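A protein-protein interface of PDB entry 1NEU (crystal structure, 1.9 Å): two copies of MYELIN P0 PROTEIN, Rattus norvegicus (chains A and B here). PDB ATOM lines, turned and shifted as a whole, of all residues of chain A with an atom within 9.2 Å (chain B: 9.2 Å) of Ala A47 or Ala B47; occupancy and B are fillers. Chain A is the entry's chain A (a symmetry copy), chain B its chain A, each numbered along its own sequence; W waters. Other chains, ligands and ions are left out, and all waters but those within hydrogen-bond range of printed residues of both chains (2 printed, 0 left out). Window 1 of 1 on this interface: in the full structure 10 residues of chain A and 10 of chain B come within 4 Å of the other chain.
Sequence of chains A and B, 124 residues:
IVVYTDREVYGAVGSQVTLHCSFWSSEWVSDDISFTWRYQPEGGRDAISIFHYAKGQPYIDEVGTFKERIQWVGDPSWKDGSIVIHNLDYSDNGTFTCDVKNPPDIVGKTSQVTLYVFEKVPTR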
ATOM      1  N   THR A  36     -24.639  10.702  12.121  1.00  0.00           N
ATOM      2  CA  THR A  36     -25.011  10.328  13.469  1.00  0.00           C
ATOM      3  C   THR A  36     -25.379  11.599  14.246  1.00  0.00           C
ATOM      4  O   THR A  36     -24.627  12.572  14.217  1.00  0.00           O
ATOM      5  CB  THR A  36     -23.863   9.620  14.213  1.00  0.00           C
ATOM      6  OG1 THR A  36     -23.420   8.471  13.464  1.00  0.00           O
ATOM      7  CG2 THR A  36     -24.329   9.182  15.630  1.00  0.00           C
ATOM      8  N   TRP A  37     -26.541  11.621  14.889  1.00  0.00           N
ATOM      9  CA  TRP A  37     -26.954  12.765  15.730  1.00  0.00           C
ATOM     10  C   TRP A  37     -26.872  12.425  17.252  1.00  0.00           C
ATOM     11  O   TRP A  37     -27.465  11.430  17.702  1.00  0.00           O
ATOM     12  CB  TRP A  37     -28.387  13.230  15.397  1.00  0.00           C
ATOM     13  CG  TRP A  37     -28.493  14.155  14.222  1.00  0.00           C
ATOM     14  CD1 TRP A  37     -28.961  13.845  12.966  1.00  0.00           C
ATOM     15  CD2 TRP A  37     -28.259  15.575  14.222  1.00  0.00           C
ATOM     16  NE1 TRP A  37     -29.051  14.987  12.196  1.00  0.00           N
ATOM     17  CE2 TRP A  37     -28.637  16.063  12.941  1.00  0.00           C
ATOM     18  CE3 TRP A  37     -27.783  16.496  15.193  1.00  0.00           C
ATOM     19  CZ2 TRP A  37     -28.560  17.426  12.608  1.00  0.00           C
ATOM     20  CZ3 TRP A  37     -27.709  17.854  14.857  1.00  0.00           C
ATOM     21  CH2 TRP A  37     -28.096  18.304  13.578  1.00  0.00           C
ATOM     22  N   ARG A  38     -26.149  13.246  18.028  1.00  0.00           N
ATOM     23  CA  ARG A  38     -26.038  13.058  19.480  1.00  0.00           C
ATOM     24  C   ARG A  38     -26.623  14.283  20.230  1.00  0.00           C
ATOM     25  O   ARG A  38     -26.613  15.413  19.716  1.00  0.00           O
ATOM     26  CB  ARG A  38     -24.582  12.812  19.886  1.00  0.00           C
ATOM     27  CG  ARG A  38     -24.073  11.420  19.583  1.00  0.00           C
ATOM     28  CD  ARG A  38     -22.598  11.281  19.914  1.00  0.00           C
ATOM     29  NE  ARG A  38     -22.074   9.989  19.465  1.00  0.00           N
ATOM     30  CZ  ARG A  38     -21.484   9.777  18.278  1.00  0.00           C
ATOM     31  NH1 ARG A  38     -21.319  10.780  17.390  1.00  0.00           N
ATOM     32  NH2 ARG A  38     -21.067   8.548  17.969  1.00  0.00           N
ATOM     33  N   TYR A  39     -27.177  14.048  21.417  1.00  0.00           N
ATOM     34  CA  TYR A  39     -27.809  15.085  22.234  1.00  0.00           C
ATOM     35  C   TYR A  39     -27.199  15.192  23.652  1.00  0.00           C
ATOM     36  O   TYR A  39     -26.991  14.176  24.321  1.00  0.00           O
ATOM     37  CB  TYR A  39     -29.312  14.784  22.355  1.00  0.00           C
ATOM     38  CG  TYR A  39     -30.069  15.640  23.368  1.00  0.00           C
ATOM     39  CD1 TYR A  39     -30.320  16.990  23.116  1.00  0.00           C
ATOM     40  CD2 TYR A  39     -30.556  15.096  24.570  1.00  0.00           C
ATOM     41  CE1 TYR A  39     -31.046  17.791  24.033  1.00  0.00           C
ATOM     42  CE2 TYR A  39     -31.272  15.888  25.497  1.00  0.00           C
ATOM     43  CZ  TYR A  39     -31.508  17.231  25.207  1.00  0.00           C
ATOM     44  OH  TYR A  39     -32.206  18.043  26.074  1.00  0.00           O
ATOM     45  N   GLN A  40     -26.932  16.434  24.082  1.00  0.00           N
ATOM     46  CA  GLN A  40     -26.403  16.748  25.417  1.00  0.00           C
ATOM     47  C   GLN A  40     -27.356  17.775  26.063  1.00  0.00           C
ATOM     48  O   GLN A  40     -27.481  18.904  25.580  1.00  0.00           O
ATOM     49  CB  GLN A  40     -24.998  17.343  25.307  1.00  0.00           C
ATOM     50  CG  GLN A  40     -24.392  17.668  26.674  1.00  0.00           C
ATOM     51  CD  GLN A  40     -22.996  18.264  26.574  1.00  0.00           C
ATOM     52  OE1 GLN A  40     -21.995  17.532  26.438  1.00  0.00           O
ATOM     53  NE2 GLN A  40     -22.909  19.586  26.649  1.00  0.00           N
ATOM     54  N   PRO A  41     -28.092  17.386  27.116  1.00  0.00           N
ATOM     55  CA  PRO A  41     -29.003  18.355  27.739  1.00  0.00           C
ATOM     56  C   PRO A  41     -28.289  19.562  28.358  1.00  0.00           C
ATOM     57  O   PRO A  41     -27.100  19.498  28.722  1.00  0.00           O
ATOM     58  CB  PRO A  41     -29.735  17.530  28.793  1.00  0.00           C
ATOM     59  CG  PRO A  41     -28.778  16.462  29.121  1.00  0.00           C
ATOM     60  CD  PRO A  41     -28.158  16.089  27.800  1.00  0.00           C
ATOM     61  N   GLY A  44     -25.441  19.524  31.044  1.00  0.00           N
ATOM     62  CA  GLY A  44     -24.908  18.177  31.201  1.00  0.00           C
ATOM     63  C   GLY A  44     -23.641  18.038  30.381  1.00  0.00           C
ATOM     64  O   GLY A  44     -23.254  18.978  29.683  1.00  0.00           O
ATOM     65  N   ARG A  45     -22.956  16.904  30.495  1.00  0.00           N
ATOM     66  CA  ARG A  45     -21.756  16.678  29.693  1.00  0.00           C
ATOM     67  C   ARG A  45     -21.749  15.358  28.889  1.00  0.00           C
ATOM     68  O   ARG A  45     -20.761  15.057  28.208  1.00  0.00           O
ATOM     69  CB  ARG A  45     -20.480  16.831  30.523  1.00  0.00           C
ATOM     70  CG  ARG A  45     -20.104  18.287  30.760  1.00  0.00           C
ATOM     71  CD  ARG A  45     -18.711  18.413  31.344  1.00  0.00           C
ATOM     72  NE  ARG A  45     -18.694  18.016  32.745  1.00  0.00           N
ATOM     73  CZ  ARG A  45     -18.957  18.851  33.752  1.00  0.00           C
ATOM     74  NH1 ARG A  45     -19.244  20.133  33.493  1.00  0.00           N
ATOM     75  NH2 ARG A  45     -18.969  18.405  35.012  1.00  0.00           N
ATOM     76  N   ASP A  46     -22.838  14.591  28.970  1.00  0.00           N
ATOM     77  CA  ASP A  46     -22.985  13.320  28.242  1.00  0.00           C
ATOM     78  C   ASP A  46     -23.649  13.493  26.882  1.00  0.00           C
ATOM     79  O   ASP A  46     -24.739  14.042  26.824  1.00  0.00           O
ATOM     80  CB  ASP A  46     -23.883  12.386  29.022  1.00  0.00           C
ATOM     81  CG  ASP A  46     -23.209  11.795  30.203  1.00  0.00           C
ATOM     82  OD1 ASP A  46     -21.998  12.043  30.416  1.00  0.00           O
ATOM     83  OD2 ASP A  46     -23.902  11.052  30.928  1.00  0.00           O
ATOM     84  N   ALA A  47     -23.060  12.955  25.814  1.00  0.00           N
ATOM     85  CA  ALA A  47     -23.660  13.067  24.461  1.00  0.00           C
ATOM     86  C   ALA A  47     -24.291  11.732  24.035  1.00  0.00           C
ATOM     87  O   ALA A  47     -23.568  10.782  23.681  1.00  0.00           O
ATOM     88  CB  ALA A  47     -22.607  13.496  23.465  1.00  0.00           C
ATOM     89  N   ILE A  48     -25.624  11.649  24.055  1.00  0.00           N
ATOM     90  CA  ILE A  48     -26.344  10.412  23.722  1.00  0.00           C
ATOM     91  C   ILE A  48     -26.790  10.375  22.251  1.00  0.00           C
ATOM     92  O   ILE A  48     -27.334  11.359  21.769  1.00  0.00           O
ATOM     93  CB  ILE A  48     -27.568  10.232  24.669  1.00  0.00           C
ATOM     94  CG1 ILE A  48     -27.089  10.312  26.120  1.00  0.00           C
ATOM     95  CG2 ILE A  48     -28.247   8.899  24.473  1.00  0.00           C
ATOM     96  CD1 ILE A  48     -25.909   9.356  26.450  1.00  0.00           C
ATOM     97  N   SER A  49     -26.544   9.253  21.555  1.00  0.00           N
ATOM     98  CA  SER A  49     -26.926   9.116  20.138  1.00  0.00           C
ATOM     99  C   SER A  49     -28.437   8.927  20.024  1.00  0.00           C
ATOM    100  O   SER A  49     -29.029   8.175  20.794  1.00  0.00           O
ATOM    101  CB  SER A  49     -26.192   7.906  19.513  1.00  0.00           C
ATOM    102  OG  SER A  49     -26.620   7.617  18.184  1.00  0.00           O
ATOM    103  N   ILE A  50     -29.077   9.712  19.157  1.00  0.00           N
ATOM    104  CA  ILE A  50     -30.533   9.623  18.968  1.00  0.00           C
ATOM    105  C   ILE A  50     -30.940   9.166  17.549  1.00  0.00           C
ATOM    106  O   ILE A  50     -32.087   8.710  17.336  1.00  0.00           O
ATOM    107  CB  ILE A  50     -31.237  10.957  19.295  1.00  0.00           C
ATOM    108  CG1 ILE A  50     -30.974  11.997  18.196  1.00  0.00           C
ATOM    109  CG2 ILE A  50     -30.769  11.460  20.712  1.00  0.00           C
ATOM    110  CD1 ILE A  50     -31.695  13.338  18.398  1.00  0.00           C
ATOM    111  N   THR A  95     -27.746  20.894  23.487  1.00  0.00           N
ATOM    112  CA  THR A  95     -26.929  20.992  22.291  1.00  0.00           C
ATOM    113  C   THR A  95     -26.946  19.664  21.501  1.00  0.00           C
ATOM    114  O   THR A  95     -26.741  18.593  22.084  1.00  0.00           O
ATOM    115  CB  THR A  95     -25.468  21.373  22.659  1.00  0.00           C
ATOM    116  OG1 THR A  95     -25.477  22.635  23.338  1.00  0.00           O
ATOM    117  CG2 THR A  95     -24.585  21.490  21.400  1.00  0.00           C
ATOM    118  N   PHE A  96     -27.193  19.760  20.192  1.00  0.00           N
ATOM    119  CA  PHE A  96     -27.219  18.598  19.269  1.00  0.00           C
ATOM    120  C   PHE A  96     -25.993  18.657  18.372  1.00  0.00           C
ATOM    121  O   PHE A  96     -25.635  19.718  17.868  1.00  0.00           O
ATOM    122  CB  PHE A  96     -28.460  18.616  18.350  1.00  0.00           C
ATOM    123  CG  PHE A  96     -29.756  18.466  19.070  1.00  0.00           C
ATOM    124  CD1 PHE A  96     -30.355  19.565  19.698  1.00  0.00           C
ATOM    125  CD2 PHE A  96     -30.375  17.219  19.143  1.00  0.00           C
ATOM    126  CE1 PHE A  96     -31.563  19.432  20.401  1.00  0.00           C
ATOM    127  CE2 PHE A  96     -31.584  17.063  19.839  1.00  0.00           C
ATOM    128  CZ  PHE A  96     -32.182  18.175  20.473  1.00  0.00           C
ATOM    129  N   THR A  97     -25.342  17.522  18.184  1.00  0.00           N
ATOM    130  CA  THR A  97     -24.172  17.465  17.310  1.00  0.00           C
ATOM    131  C   THR A  97     -24.333  16.452  16.144  1.00  0.00           C
ATOM    132  O   THR A  97     -24.696  15.279  16.350  1.00  0.00           O
ATOM    133  CB  THR A  97     -22.875  17.098  18.109  1.00  0.00           C
ATOM    134  OG1 THR A  97     -22.713  18.011  19.208  1.00  0.00           O
ATOM    135  CG2 THR A  97     -21.640  17.189  17.196  1.00  0.00           C
ATOM    136  N   ASP A  99     -22.437  14.381  13.275  1.00  0.00           N
ATOM    137  CA  ASP A  99     -21.147  13.729  12.986  1.00  0.00           C
ATOM    138  C   ASP A  99     -21.233  13.029  11.617  1.00  0.00           C
ATOM    139  O   ASP A  99     -22.010  12.069  11.431  1.00  0.00           O
ATOM    140  CB  ASP A  99     -20.893  12.709  14.114  1.00  0.00           C
ATOM    141  CG  ASP A  99     -19.533  12.000  14.027  1.00  0.00           C
ATOM    142  OD1 ASP A  99     -18.729  12.174  13.073  1.00  0.00           O
ATOM    143  OD2 ASP A  99     -19.289  11.198  14.959  1.00  0.00           O
ATOM    144  N   GLN A 112     -22.264  21.512  15.727  1.00  0.00           N
ATOM    145  CA  GLN A 112     -23.360  21.515  16.707  1.00  0.00           C
ATOM    146  C   GLN A 112     -24.307  22.704  16.578  1.00  0.00           C
ATOM    147  O   GLN A 112     -23.964  23.718  15.984  1.00  0.00           O
ATOM    148  CB  GLN A 112     -22.799  21.436  18.145  1.00  0.00           C
ATOM    149  CG  GLN A 112     -21.843  22.561  18.491  1.00  0.00           C
ATOM    150  CD  GLN A 112     -21.369  22.551  19.953  1.00  0.00           C
ATOM    151  OE1 GLN A 112     -21.301  23.607  20.608  1.00  0.00           O
ATOM    152  NE2 GLN A 112     -21.085  21.372  20.476  1.00  0.00           N
ATOM    153  N   THR B  36     -12.247  17.898  29.081  1.00  0.00           N
ATOM    154  CA  THR B  36     -13.324  16.968  29.344  1.00  0.00           C
ATOM    155  C   THR B  36     -13.015  15.645  28.633  1.00  0.00           C
ATOM    156  O   THR B  36     -12.677  15.652  27.450  1.00  0.00           O
ATOM    157  CB  THR B  36     -14.680  17.489  28.832  1.00  0.00           C
ATOM    158  OG1 THR B  36     -14.964  18.781  29.404  1.00  0.00           O
ATOM    159  CG2 THR B  36     -15.813  16.488  29.194  1.00  0.00           C
ATOM    160  N   TRP B  37     -13.072  14.525  29.346  1.00  0.00           N
ATOM    161  CA  TRP B  37     -12.868  13.193  28.738  1.00  0.00           C
ATOM    162  C   TRP B  37     -14.209  12.401  28.616  1.00  0.00           C
ATOM    163  O   TRP B  37     -14.921  12.221  29.618  1.00  0.00           O
ATOM    164  CB  TRP B  37     -11.857  12.348  29.541  1.00  0.00           C
ATOM    165  CG  TRP B  37     -10.417  12.624  29.231  1.00  0.00           C
ATOM    166  CD1 TRP B  37      -9.522  13.318  30.012  1.00  0.00           C
ATOM    167  CD2 TRP B  37      -9.659  12.096  28.128  1.00  0.00           C
ATOM    168  NE1 TRP B  37      -8.255  13.235  29.473  1.00  0.00           N
ATOM    169  CE2 TRP B  37      -8.306  12.486  28.324  1.00  0.00           C
ATOM    170  CE3 TRP B  37      -9.988  11.308  26.992  1.00  0.00           C
ATOM    171  CZ2 TRP B  37      -7.284  12.111  27.435  1.00  0.00           C
ATOM    172  CZ3 TRP B  37      -8.966  10.936  26.110  1.00  0.00           C
ATOM    173  CH2 TRP B  37      -7.633  11.337  26.337  1.00  0.00           C
ATOM    174  N   ARG B  38     -14.539  11.933  27.403  1.00  0.00           N
ATOM    175  CA  ARG B  38     -15.748  11.134  27.173  1.00  0.00           C
ATOM    176  C   ARG B  38     -15.371   9.721  26.654  1.00  0.00           C
ATOM    177  O   ARG B  38     -14.332   9.535  26.001  1.00  0.00           O
ATOM    178  CB  ARG B  38     -16.690  11.841  26.195  1.00  0.00           C
ATOM    179  CG  ARG B  38     -17.466  12.994  26.795  1.00  0.00           C
ATOM    180  CD  ARG B  38     -18.296  13.712  25.747  1.00  0.00           C
ATOM    181  NE  ARG B  38     -18.912  14.922  26.297  1.00  0.00           N
ATOM    182  CZ  ARG B  38     -18.373  16.150  26.228  1.00  0.00           C
ATOM    183  NH1 ARG B  38     -17.189  16.360  25.616  1.00  0.00           N
ATOM    184  NH2 ARG B  38     -19.016  17.175  26.790  1.00  0.00           N
ATOM    185  N   TYR B  39     -16.186   8.724  26.990  1.00  0.00           N
ATOM    186  CA  TYR B  39     -15.953   7.328  26.618  1.00  0.00           C
ATOM    187  C   TYR B  39     -17.135   6.706  25.836  1.00  0.00           C
ATOM    188  O   TYR B  39     -18.295   6.866  26.225  1.00  0.00           O
ATOM    189  CB  TYR B  39     -15.702   6.502  27.889  1.00  0.00           C
ATOM    190  CG  TYR B  39     -15.676   4.988  27.690  1.00  0.00           C
ATOM    191  CD1 TYR B  39     -14.609   4.373  27.033  1.00  0.00           C
ATOM    192  CD2 TYR B  39     -16.708   4.166  28.177  1.00  0.00           C
ATOM    193  CE1 TYR B  39     -14.556   2.967  26.866  1.00  0.00           C
ATOM    194  CE2 TYR B  39     -16.671   2.763  28.006  1.00  0.00           C
ATOM    195  CZ  TYR B  39     -15.586   2.185  27.351  1.00  0.00           C
ATOM    196  OH  TYR B  39     -15.499   0.822  27.164  1.00  0.00           O
ATOM    197  N   GLN B  40     -16.808   5.999  24.744  1.00  0.00           N
ATOM    198  CA  GLN B  40     -17.778   5.287  23.901  1.00  0.00           C
ATOM    199  C   GLN B  40     -17.316   3.819  23.801  1.00  0.00           C
ATOM    200  O   GLN B  40     -16.254   3.534  23.241  1.00  0.00           O
ATOM    201  CB  GLN B  40     -17.829   5.911  22.504  1.00  0.00           C
ATOM    202  CG  GLN B  40     -18.843   5.218  21.592  1.00  0.00           C
ATOM    203  CD  GLN B  40     -18.899   5.829  20.200  1.00  0.00           C
ATOM    204  OE1 GLN B  40     -19.576   6.853  19.976  1.00  0.00           O
ATOM    205  NE2 GLN B  40     -18.203   5.212  19.254  1.00  0.00           N
ATOM    206  N   PRO B  41     -18.062   2.875  24.396  1.00  0.00           N
ATOM    207  CA  PRO B  41     -17.631   1.473  24.308  1.00  0.00           C
ATOM    208  C   PRO B  41     -17.616   0.923  22.877  1.00  0.00           C
ATOM    209  O   PRO B  41     -18.328   1.416  21.983  1.00  0.00           O
ATOM    210  CB  PRO B  41     -18.636   0.736  25.186  1.00  0.00           C
ATOM    211  CG  PRO B  41     -19.836   1.586  25.128  1.00  0.00           C
ATOM    212  CD  PRO B  41     -19.304   2.995  25.168  1.00  0.00           C
ATOM    213  N   GLY B  44     -20.578   0.858  20.318  1.00  0.00           N
ATOM    214  CA  GLY B  44     -21.672   1.701  20.784  1.00  0.00           C
ATOM    215  C   GLY B  44     -21.590   3.053  20.105  1.00  0.00           C
ATOM    216  O   GLY B  44     -20.659   3.299  19.336  1.00  0.00           O
ATOM    217  N   ARG B  45     -22.579   3.914  20.328  1.00  0.00           N
ATOM    218  CA  ARG B  45     -22.539   5.255  19.751  1.00  0.00           C
ATOM    219  C   ARG B  45     -22.734   6.406  20.765  1.00  0.00           C
ATOM    220  O   ARG B  45     -22.754   7.579  20.368  1.00  0.00           O
ATOM    221  CB  ARG B  45     -23.493   5.392  18.564  1.00  0.00           C
ATOM    222  CG  ARG B  45     -22.936   4.776  17.287  1.00  0.00           C
ATOM    223  CD  ARG B  45     -23.766   5.156  16.078  1.00  0.00           C
ATOM    224  NE  ARG B  45     -25.029   4.431  16.063  1.00  0.00           N
ATOM    225  CZ  ARG B  45     -25.182   3.224  15.518  1.00  0.00           C
ATOM    226  NH1 ARG B  45     -24.137   2.623  14.934  1.00  0.00           N
ATOM    227  NH2 ARG B  45     -26.361   2.598  15.583  1.00  0.00           N
ATOM    228  N   ASP B  46     -22.872   6.070  22.048  1.00  0.00           N
ATOM    229  CA  ASP B  46     -23.040   7.057  23.127  1.00  0.00           C
ATOM    230  C   ASP B  46     -21.717   7.477  23.753  1.00  0.00           C
ATOM    231  O   ASP B  46     -20.975   6.614  24.199  1.00  0.00           O
ATOM    232  CB  ASP B  46     -23.852   6.452  24.250  1.00  0.00           C
ATOM    233  CG  ASP B  46     -25.295   6.351  23.924  1.00  0.00           C
ATOM    234  OD1 ASP B  46     -25.721   6.810  22.837  1.00  0.00           O
ATOM    235  OD2 ASP B  46     -26.026   5.814  24.782  1.00  0.00           O
ATOM    236  N   ALA B  47     -21.457   8.779  23.877  1.00  0.00           N
ATOM    237  CA  ALA B  47     -20.197   9.261  24.495  1.00  0.00           C
ATOM    238  C   ALA B  47     -20.457   9.794  25.914  1.00  0.00           C
ATOM    239  O   ALA B  47     -21.009  10.898  26.076  1.00  0.00           O
ATOM    240  CB  ALA B  47     -19.578  10.336  23.632  1.00  0.00           C
ATOM    241  N   ILE B  48     -20.063   9.032  26.937  1.00  0.00           N
ATOM    242  CA  ILE B  48     -20.303   9.405  28.338  1.00  0.00           C
ATOM    243  C   ILE B  48     -19.097  10.127  28.964  1.00  0.00           C
ATOM    244  O   ILE B  48     -17.978   9.660  28.805  1.00  0.00           O
ATOM    245  CB  ILE B  48     -20.680   8.145  29.172  1.00  0.00           C
ATOM    246  CG1 ILE B  48     -21.857   7.437  28.498  1.00  0.00           C
ATOM    247  CG2 ILE B  48     -21.091   8.497  30.581  1.00  0.00           C
ATOM    248  CD1 ILE B  48     -23.068   8.365  28.202  1.00  0.00           C
ATOM    249  N   SER B  49     -19.337  11.255  29.653  1.00  0.00           N
ATOM    250  CA  SER B  49     -18.251  12.024  30.287  1.00  0.00           C
ATOM    251  C   SER B  49     -17.760  11.295  31.536  1.00  0.00           C
ATOM    252  O   SER B  49     -18.563  10.792  32.318  1.00  0.00           O
ATOM    253  CB  SER B  49     -18.761  13.435  30.664  1.00  0.00           C
ATOM    254  OG  SER B  49     -17.815  14.191  31.416  1.00  0.00           O
ATOM    255  N   ILE B  50     -16.443  11.118  31.651  1.00  0.00           N
ATOM    256  CA  ILE B  50     -15.858  10.425  32.807  1.00  0.00           C
ATOM    257  C   ILE B  50     -14.951  11.331  33.672  1.00  0.00           C
ATOM    258  O   ILE B  50     -14.671  11.007  34.849  1.00  0.00           O
ATOM    259  CB  ILE B  50     -15.067   9.169  32.384  1.00  0.00           C
ATOM    260  CG1 ILE B  50     -13.740   9.559  31.715  1.00  0.00           C
ATOM    261  CG2 ILE B  50     -15.965   8.279  31.446  1.00  0.00           C
ATOM    262  CD1 ILE B  50     -12.849   8.372  31.322  1.00  0.00           C
ATOM    263  N   THR B  95     -13.459   3.820  22.520  1.00  0.00           N
ATOM    264  CA  THR B  95     -12.809   5.042  22.083  1.00  0.00           C
ATOM    265  C   THR B  95     -13.010   6.173  23.116  1.00  0.00           C
ATOM    266  O   THR B  95     -14.139   6.413  23.561  1.00  0.00           O
ATOM    267  CB  THR B  95     -13.354   5.485  20.697  1.00  0.00           C
ATOM    268  OG1 THR B  95     -13.102   4.442  19.747  1.00  0.00           O
ATOM    269  CG2 THR B  95     -12.670   6.778  20.212  1.00  0.00           C
ATOM    270  N   PHE B  96     -11.913   6.842  23.479  1.00  0.00           N
ATOM    271  CA  PHE B  96     -11.916   7.978  24.435  1.00  0.00           C
ATOM    272  C   PHE B  96     -11.648   9.264  23.669  1.00  0.00           C
ATOM    273  O   PHE B  96     -10.776   9.309  22.805  1.00  0.00           O
ATOM    274  CB  PHE B  96     -10.808   7.840  25.502  1.00  0.00           C
ATOM    275  CG  PHE B  96     -10.978   6.673  26.411  1.00  0.00           C
ATOM    276  CD1 PHE B  96     -10.581   5.391  26.009  1.00  0.00           C
ATOM    277  CD2 PHE B  96     -11.554   6.843  27.669  1.00  0.00           C
ATOM    278  CE1 PHE B  96     -10.757   4.278  26.846  1.00  0.00           C
ATOM    279  CE2 PHE B  96     -11.739   5.746  28.524  1.00  0.00           C
ATOM    280  CZ  PHE B  96     -11.339   4.455  28.111  1.00  0.00           C
ATOM    281  N   THR B  97     -12.405  10.304  23.975  1.00  0.00           N
ATOM    282  CA  THR B  97     -12.202  11.595  23.322  1.00  0.00           C
ATOM    283  C   THR B  97     -11.893  12.741  24.324  1.00  0.00           C
ATOM    284  O   THR B  97     -12.612  12.941  25.321  1.00  0.00           O
ATOM    285  CB  THR B  97     -13.448  12.008  22.466  1.00  0.00           C
ATOM    286  OG1 THR B  97     -13.767  10.954  21.542  1.00  0.00           O
ATOM    287  CG2 THR B  97     -13.152  13.295  21.676  1.00  0.00           C
ATOM    288  N   ASP B  99     -11.673  16.717  24.839  1.00  0.00           N
ATOM    289  CA  ASP B  99     -12.291  17.973  24.379  1.00  0.00           C
ATOM    290  C   ASP B  99     -11.675  19.150  25.159  1.00  0.00           C
ATOM    291  O   ASP B  99     -11.838  19.263  26.392  1.00  0.00           O
ATOM    292  CB  ASP B  99     -13.805  17.860  24.653  1.00  0.00           C
ATOM    293  CG  ASP B  99     -14.626  19.053  24.142  1.00  0.00           C
ATOM    294  OD1 ASP B  99     -14.104  20.073  23.619  1.00  0.00           O
ATOM    295  OD2 ASP B  99     -15.864  18.961  24.315  1.00  0.00           O
ATOM    296  N   GLN B 112      -9.312  11.865  19.567  1.00  0.00           N
ATOM    297  CA  GLN B 112      -9.649  10.573  20.182  1.00  0.00           C
ATOM    298  C   GLN B 112      -8.528   9.541  20.117  1.00  0.00           C
ATOM    299  O   GLN B 112      -7.613   9.659  19.311  1.00  0.00           O
ATOM    300  CB  GLN B 112     -10.938   9.996  19.554  1.00  0.00           C
ATOM    301  CG  GLN B 112     -10.855   9.807  18.052  1.00  0.00           C
ATOM    302  CD  GLN B 112     -12.091   9.131  17.438  1.00  0.00           C
ATOM    303  OE1 GLN B 112     -11.970   8.246  16.571  1.00  0.00           O
ATOM    304  NE2 GLN B 112     -13.267   9.507  17.907  1.00  0.00           N
HETATM  305  O   HOH W   1     -28.814   5.966  22.612  1.00  0.00           O
HETATM  306  O   HOH W   2     -21.269  10.759  33.271  1.00  0.00           O
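Water W2 bridges the backbone carbonyl oxygen of Ser B49 and the side-chain carboxylate of Asp A46.
Water W1 lies within hydrogen-bond range of the backbone carbonyl oxygen (O) of Ser A49 (2.9 Å) and the side-chain carboxylate (OD1) of Asp B46 (3.2 Å).
Arg A38 touches Gln B40, and with the chains exchanged Gln A40 touches Arg B38.
Arg A38 touches Arg B45, and with the chains exchanged Arg A45 touches Arg B38.
Arg A45 touches Ser B49, and with the chains exchanged Ser A49 touches Arg B45.
Asp A46 touches Ser B49, and with the chains exchanged Ser A49 touches Asp B46.
Hydrophobic or aromatic side chains of chain A that line the printed part of chain B: Ile A48.
Of the 18 printed residues of chain B, 7 touch a printed residue of chain A.
The side-chain amide oxygen of Gln A40 sits at hydrogen-bond distance from the guanidinium group of Arg B38.
The guanidinium group (NE) of Arg B38 is in hydrogen-bond range of the backbone carbonyl oxygen (O) of Arg A45, at 2.7 Å.
The guanidinium group (NH2) of Arg A38 sits at hydrogen-bond distance from the side-chain amide oxygen (OE1) of Gln B40.
NE of Arg A38 lies within hydrogen-bond range of O of Arg B45, at 2.7 Å.
The side-chain carboxylate (OD1) of Asp B46 sits at hydrogen-bond distance from the backbone NH (N) of Ser A49, 2.9 Å away.
The backbone carbonyl oxygen of Ala B47 sits at hydrogen-bond distance from the backbone NH of Ala A47.
The side-chain carboxylate of Asp A46 lies within hydrogen-bond range of the backbone NH of Ser B49.
Among the printed residues, merely in contact across the chains: Arg A45 with Ser B49 (3.6 Å), Asp A46 with Ala B47 (3.8 Å), Asp A46 with Ile B48 (3.7 Å), Ala A47 with Asp B46 (3.8 Å), Ile A48 with Asp B46 (3.7 Å), Ile A48 with Ile B48 (3.5 Å) and Ser A49 with Arg B45 (3.6 Å).
Ala A47 touches just these residues of chain B: Asp B46 and Ala B47.
Ile B48 touches just these residues of chain A: Asp A46 (3.7 Å) and Ile A48 (3.5 Å).
Of the printed residues of chain B, Arg A45 touches Arg B38 and Ser B49.
Of the printed residues of chain A, Gln B40 touches Arg A38.
Of the printed residues of chain A, Asp B46 touches Ala A47, Ile A48 and Ser A49.
Of the printed residues of chain B, Ser A49 touches Arg B45 (3.6 Å) and Asp B46 (2.9 Å).
Tyr B39 touches none of the printed residues of chain A.
Asp A99 touches none of the printed residues of chain B.
The nearest residue of chain A that does not touch Ala B47 is Arg A38 (4.6 Å).
The side-chain carboxylate (OD2) of Asp B99 is in salt-bridge range of the guanidinium group (NH1) of Arg B38, at 3.2 Å.
NH1 of Arg A38 lies within salt-bridge range of OD2 of Asp A99, at 3.2 Å.
The side-chain amide nitrogen (NE2) of Gln A40 sits at hydrogen-bond distance from the backbone carbonyl oxygen (O) of Gly A44 (3.1 Å).
The backbone carbonyl oxygen (O) of Arg A45 lies close to the side-chain amide oxygen (OE1) of Gln A40 (3.3 Å).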
